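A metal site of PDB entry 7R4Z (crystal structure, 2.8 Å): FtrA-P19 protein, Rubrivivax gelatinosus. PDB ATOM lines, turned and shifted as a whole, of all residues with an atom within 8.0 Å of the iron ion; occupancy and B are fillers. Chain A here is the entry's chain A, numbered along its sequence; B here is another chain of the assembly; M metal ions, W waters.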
ATOM      1  N   GLU A  25     -11.663  26.096 -17.959  1.00  0.00           N
ATOM      2  CA  GLU A  25     -12.573  27.215 -17.860  1.00  0.00           C
ATOM      3  C   GLU A  25     -11.852  28.438 -18.392  1.00  0.00           C
ATOM      4  O   GLU A  25     -10.620  28.539 -18.320  1.00  0.00           O
ATOM      5  CB  GLU A  25     -13.000  27.414 -16.400  1.00  0.00           C
ATOM      6  CG  GLU A  25     -13.878  26.301 -15.859  1.00  0.00           C
ATOM      7  CD  GLU A  25     -14.333  26.446 -14.418  1.00  0.00           C
ATOM      8  OE1 GLU A  25     -13.707  27.221 -13.648  1.00  0.00           O
ATOM      9  OE2 GLU A  25     -15.306  25.742 -14.044  1.00  0.00           O
ATOM     10  N   VAL A  42     -16.880  32.855 -14.971  1.00  0.00           N
ATOM     11  CA  VAL A  42     -16.157  31.976 -15.897  1.00  0.00           C
ATOM     12  C   VAL A  42     -17.132  31.323 -16.890  1.00  0.00           C
ATOM     13  O   VAL A  42     -18.342  31.448 -16.757  1.00  0.00           O
ATOM     14  CB  VAL A  42     -15.207  30.928 -15.245  1.00  0.00           C
ATOM     15  CG1 VAL A  42     -14.368  31.551 -14.133  1.00  0.00           C
ATOM     16  CG2 VAL A  42     -15.964  29.719 -14.732  1.00  0.00           C
ATOM     17  N   TYR A  43     -16.576  30.679 -17.914  1.00  0.00           N
ATOM     18  CA  TYR A  43     -17.337  29.863 -18.842  1.00  0.00           C
ATOM     19  C   TYR A  43     -16.517  28.659 -19.243  1.00  0.00           C
ATOM     20  O   TYR A  43     -15.280  28.671 -19.170  1.00  0.00           O
ATOM     21  CB  TYR A  43     -17.885  30.618 -20.053  1.00  0.00           C
ATOM     22  CG  TYR A  43     -16.831  31.071 -21.040  1.00  0.00           C
ATOM     23  CD1 TYR A  43     -16.170  32.292 -20.869  1.00  0.00           C
ATOM     24  CD2 TYR A  43     -16.535  30.317 -22.170  1.00  0.00           C
ATOM     25  CE1 TYR A  43     -15.260  32.747 -21.811  1.00  0.00           C
ATOM     26  CE2 TYR A  43     -15.591  30.750 -23.096  1.00  0.00           C
ATOM     27  CZ  TYR A  43     -14.980  31.977 -22.922  1.00  0.00           C
ATOM     28  OH  TYR A  43     -14.059  32.447 -23.825  1.00  0.00           O
ATOM     29  N   LEU A  44     -17.223  27.623 -19.666  1.00  0.00           N
ATOM     30  CA  LEU A  44     -16.646  26.390 -20.162  1.00  0.00           C
ATOM     31  C   LEU A  44     -17.609  25.762 -21.192  1.00  0.00           C
ATOM     32  O   LEU A  44     -18.576  26.403 -21.591  1.00  0.00           O
ATOM     33  CB  LEU A  44     -16.312  25.441 -18.983  1.00  0.00           C
ATOM     34  CG  LEU A  44     -17.449  25.025 -18.049  1.00  0.00           C
ATOM     35  CD1 LEU A  44     -17.131  23.712 -17.391  1.00  0.00           C
ATOM     36  CD2 LEU A  44     -17.788  26.121 -17.029  1.00  0.00           C
ATOM     37  N   HIS A  64     -21.326  27.082 -20.999  1.00  0.00           N
ATOM     38  CA  HIS A  64     -21.911  26.967 -19.697  1.00  0.00           C
ATOM     39  C   HIS A  64     -21.301  28.128 -18.943  1.00  0.00           C
ATOM     40  O   HIS A  64     -20.078  28.119 -18.719  1.00  0.00           O
ATOM     41  CB  HIS A  64     -21.563  25.626 -19.037  1.00  0.00           C
ATOM     42  CG  HIS A  64     -22.239  25.475 -17.721  1.00  0.00           C
ATOM     43  ND1 HIS A  64     -23.607  25.336 -17.632  1.00  0.00           N
ATOM     44  CD2 HIS A  64     -21.716  25.542 -16.484  1.00  0.00           C
ATOM     45  CE1 HIS A  64     -23.873  25.240 -16.338  1.00  0.00           C
ATOM     46  NE2 HIS A  64     -22.775  25.385 -15.615  1.00  0.00           N
ATOM     47  N   GLU A  66     -20.827  30.471 -15.612  1.00  0.00           N
ATOM     48  CA  GLU A  66     -20.827  30.313 -14.149  1.00  0.00           C
ATOM     49  C   GLU A  66     -20.549  31.619 -13.431  1.00  0.00           C
ATOM     50  O   GLU A  66     -19.848  32.490 -13.934  1.00  0.00           O
ATOM     51  CB  GLU A  66     -19.703  29.335 -13.720  1.00  0.00           C
ATOM     52  CG  GLU A  66     -19.781  27.907 -14.237  1.00  0.00           C
ATOM     53  CD  GLU A  66     -18.718  27.033 -13.619  1.00  0.00           C
ATOM     54  OE1 GLU A  66     -17.886  27.562 -12.844  1.00  0.00           O
ATOM     55  OE2 GLU A  66     -18.734  25.796 -13.890  1.00  0.00           O
ATOM     56  N   ALA A  67     -21.036  31.691 -12.187  1.00  0.00           N
ATOM     57  CA  ALA A  67     -20.781  32.761 -11.225  1.00  0.00           C
ATOM     58  C   ALA A  67     -20.166  32.030 -10.040  1.00  0.00           C
ATOM     59  O   ALA A  67     -20.820  31.176  -9.393  1.00  0.00           O
ATOM     60  CB  ALA A  67     -22.088  33.430 -10.810  1.00  0.00           C
ATOM     61  N   ASP A  68     -18.870  32.305  -9.787  1.00  0.00           N
ATOM     62  CA  ASP A  68     -18.138  31.746  -8.660  1.00  0.00           C
ATOM     63  C   ASP A  68     -18.090  32.800  -7.534  1.00  0.00           C
ATOM     64  O   ASP A  68     -17.319  33.760  -7.614  1.00  0.00           O
ATOM     65  CB  ASP A  68     -16.741  31.195  -9.074  1.00  0.00           C
ATOM     66  CG  ASP A  68     -16.728  30.143 -10.202  1.00  0.00           C
ATOM     67  OD1 ASP A  68     -17.638  29.269 -10.241  1.00  0.00           O
ATOM     68  OD2 ASP A  68     -15.792  30.186 -11.041  1.00  0.00           O
ATOM     69  N   HIS A  70     -17.537  33.467  -3.562  1.00  0.00           N
ATOM     70  CA  HIS A  70     -16.868  32.954  -2.365  1.00  0.00           C
ATOM     71  C   HIS A  70     -16.622  34.053  -1.365  1.00  0.00           C
ATOM     72  O   HIS A  70     -16.410  35.208  -1.733  1.00  0.00           O
ATOM     73  CB  HIS A  70     -15.574  32.244  -2.707  1.00  0.00           C
ATOM     74  CG  HIS A  70     -15.817  31.022  -3.506  1.00  0.00           C
ATOM     75  ND1 HIS A  70     -15.966  31.079  -4.882  1.00  0.00           N
ATOM     76  CD2 HIS A  70     -16.065  29.754  -3.093  1.00  0.00           C
ATOM     77  CE1 HIS A  70     -16.234  29.848  -5.250  1.00  0.00           C
ATOM     78  NE2 HIS A  70     -16.312  29.017  -4.214  1.00  0.00           N
ATOM     79  N   ALA A 113     -20.216  20.551  -9.367  1.00  0.00           N
ATOM     80  CA  ALA A 113     -19.360  19.975 -10.404  1.00  0.00           C
ATOM     81  C   ALA A 113     -18.063  19.514  -9.756  1.00  0.00           C
ATOM     82  O   ALA A 113     -17.926  19.582  -8.533  1.00  0.00           O
ATOM     83  CB  ALA A 113     -19.072  21.029 -11.472  1.00  0.00           C
ATOM     84  N   SER A 114     -17.098  19.062 -10.589  1.00  0.00           N
ATOM     85  CA  SER A 114     -15.760  18.609 -10.150  1.00  0.00           C
ATOM     86  C   SER A 114     -14.980  19.705  -9.364  1.00  0.00           C
ATOM     87  O   SER A 114     -14.256  19.380  -8.440  1.00  0.00           O
ATOM     88  CB  SER A 114     -14.974  18.106 -11.352  1.00  0.00           C
ATOM     89  OG  SER A 114     -14.981  19.083 -12.388  1.00  0.00           O
ATOM     90  N   ASP A 115     -15.191  20.999  -9.716  1.00  0.00           N
ATOM     91  CA  ASP A 115     -14.574  22.169  -9.061  1.00  0.00           C
ATOM     92  C   ASP A 115     -15.396  22.679  -7.837  1.00  0.00           C
ATOM     93  O   ASP A 115     -15.018  23.669  -7.190  1.00  0.00           O
ATOM     94  CB  ASP A 115     -14.295  23.287 -10.096  1.00  0.00           C
ATOM     95  CG  ASP A 115     -15.496  23.807 -10.863  1.00  0.00           C
ATOM     96  OD1 ASP A 115     -16.431  23.019 -11.138  1.00  0.00           O
ATOM     97  OD2 ASP A 115     -15.489  24.984 -11.230  1.00  0.00           O
ATOM     98  N   GLY A 116     -16.483  21.991  -7.509  1.00  0.00           N
ATOM     99  CA  GLY A 116     -17.338  22.328  -6.382  1.00  0.00           C
ATOM    100  C   GLY A 116     -18.640  23.021  -6.726  1.00  0.00           C
ATOM    101  O   GLY A 116     -19.006  23.125  -7.906  1.00  0.00           O
ATOM    102  N   PRO A 117     -19.366  23.511  -5.692  1.00  0.00           N
ATOM    103  CA  PRO A 117     -20.639  24.188  -5.960  1.00  0.00           C
ATOM    104  C   PRO A 117     -20.440  25.550  -6.543  1.00  0.00           C
ATOM    105  O   PRO A 117     -19.409  26.221  -6.312  1.00  0.00           O
ATOM    106  CB  PRO A 117     -21.333  24.223  -4.584  1.00  0.00           C
ATOM    107  CG  PRO A 117     -20.229  24.199  -3.604  1.00  0.00           C
ATOM    108  CD  PRO A 117     -19.071  23.483  -4.234  1.00  0.00           C
ATOM    109  N   HIS A 118     -21.470  25.980  -7.267  1.00  0.00           N
ATOM    110  CA  HIS A 118     -21.535  27.254  -7.979  1.00  0.00           C
ATOM    111  C   HIS A 118     -22.942  27.485  -8.565  1.00  0.00           C
ATOM    112  O   HIS A 118     -23.849  26.658  -8.435  1.00  0.00           O
ATOM    113  CB  HIS A 118     -20.494  27.276  -9.135  1.00  0.00           C
ATOM    114  CG  HIS A 118     -20.748  26.229 -10.177  1.00  0.00           C
ATOM    115  ND1 HIS A 118     -20.407  24.907  -9.958  1.00  0.00           N
ATOM    116  CD2 HIS A 118     -21.365  26.338 -11.375  1.00  0.00           C
ATOM    117  CE1 HIS A 118     -20.813  24.251 -11.027  1.00  0.00           C
ATOM    118  NE2 HIS A 118     -21.389  25.077 -11.915  1.00  0.00           N
ATOM    119  N   TYR A 119     -23.076  28.620  -9.236  1.00  0.00           N
ATOM    120  CA  TYR A 119     -24.253  29.034  -9.969  1.00  0.00           C
ATOM    121  C   TYR A 119     -23.845  28.956 -11.446  1.00  0.00           C
ATOM    122  O   TYR A 119     -22.707  29.252 -11.781  1.00  0.00           O
ATOM    123  CB  TYR A 119     -24.674  30.451  -9.546  1.00  0.00           C
ATOM    124  CG  TYR A 119     -24.955  30.537  -8.060  1.00  0.00           C
ATOM    125  CD1 TYR A 119     -26.174  30.113  -7.530  1.00  0.00           C
ATOM    126  CD2 TYR A 119     -23.964  30.966  -7.166  1.00  0.00           C
ATOM    127  CE1 TYR A 119     -26.432  30.154  -6.150  1.00  0.00           C
ATOM    128  CE2 TYR A 119     -24.211  31.015  -5.784  1.00  0.00           C
ATOM    129  CZ  TYR A 119     -25.437  30.582  -5.280  1.00  0.00           C
ATOM    130  OH  TYR A 119     -25.662  30.585  -3.925  1.00  0.00           O
ATOM    131  N   HIS B 154     -23.567  18.145 -12.057  1.00  0.00           N
ATOM    132  CA  HIS B 154     -22.999  17.869 -13.394  1.00  0.00           C
ATOM    133  C   HIS B 154     -22.806  16.370 -13.520  1.00  0.00           C
ATOM    134  O   HIS B 154     -22.391  15.705 -12.564  1.00  0.00           O
ATOM    135  CB  HIS B 154     -21.639  18.545 -13.620  1.00  0.00           C
ATOM    136  CG  HIS B 154     -21.692  20.038 -13.755  1.00  0.00           C
ATOM    137  ND1 HIS B 154     -20.684  20.721 -14.395  1.00  0.00           N
ATOM    138  CD2 HIS B 154     -22.602  20.926 -13.281  1.00  0.00           C
ATOM    139  CE1 HIS B 154     -21.026  22.005 -14.326  1.00  0.00           C
ATOM    140  NE2 HIS B 154     -22.163  22.175 -13.668  1.00  0.00           N
ATOM    141  N   THR B 159     -16.681  17.532 -16.191  1.00  0.00           N
ATOM    142  CA  THR B 159     -16.971  18.258 -14.952  1.00  0.00           C
ATOM    143  C   THR B 159     -17.897  17.513 -13.975  1.00  0.00           C
ATOM    144  O   THR B 159     -18.164  18.014 -12.883  1.00  0.00           O
ATOM    145  CB  THR B 159     -17.510  19.654 -15.315  1.00  0.00           C
ATOM    146  OG1 THR B 159     -18.667  19.499 -16.143  1.00  0.00           O
ATOM    147  CG2 THR B 159     -16.485  20.510 -16.002  1.00  0.00           C
HETATM  148 FE    FE M   1     -16.293  26.285 -12.009  1.00  0.00          FE
HETATM  149 CU    CU M   2     -22.871  24.469 -13.451  1.00  0.00          CU
HETATM  150  O   HOH W   1     -14.197  27.431 -11.013  1.00  0.00           O
HETATM  151  O   HOH W   2     -17.396  25.995  -9.291  1.00  0.00           O
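The backbone NH (N) of Glu 66 sits at hydrogen-bond distance from the backbone carbonyl oxygen (O) of Val 42 (2.9 Å). The side-chain carboxylate (OE2) of Glu 66 lies close to a ring nitrogen (NE2) of His 118, 3.4 Å away.
Asp 68 touches the iron ion (OD1 to FE, 3.7 Å). Of the 18 residues printed, 4 come within 4 Å of the iron ion.
The iron ion is bound by OD2 of Asp 115 (1.7 Å), OE1 of Glu 66 (2.2 Å), OE2 of Glu 25 (2.3 Å) and water W1 (2.6 Å).
Water W1 lies within hydrogen-bond range of OE1 of Glu 25 and OD2 of Asp 68. Water W2 bridges ND1 of His 118 (3.3 Å) and OD1 of Asp 68 (3.4 Å).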
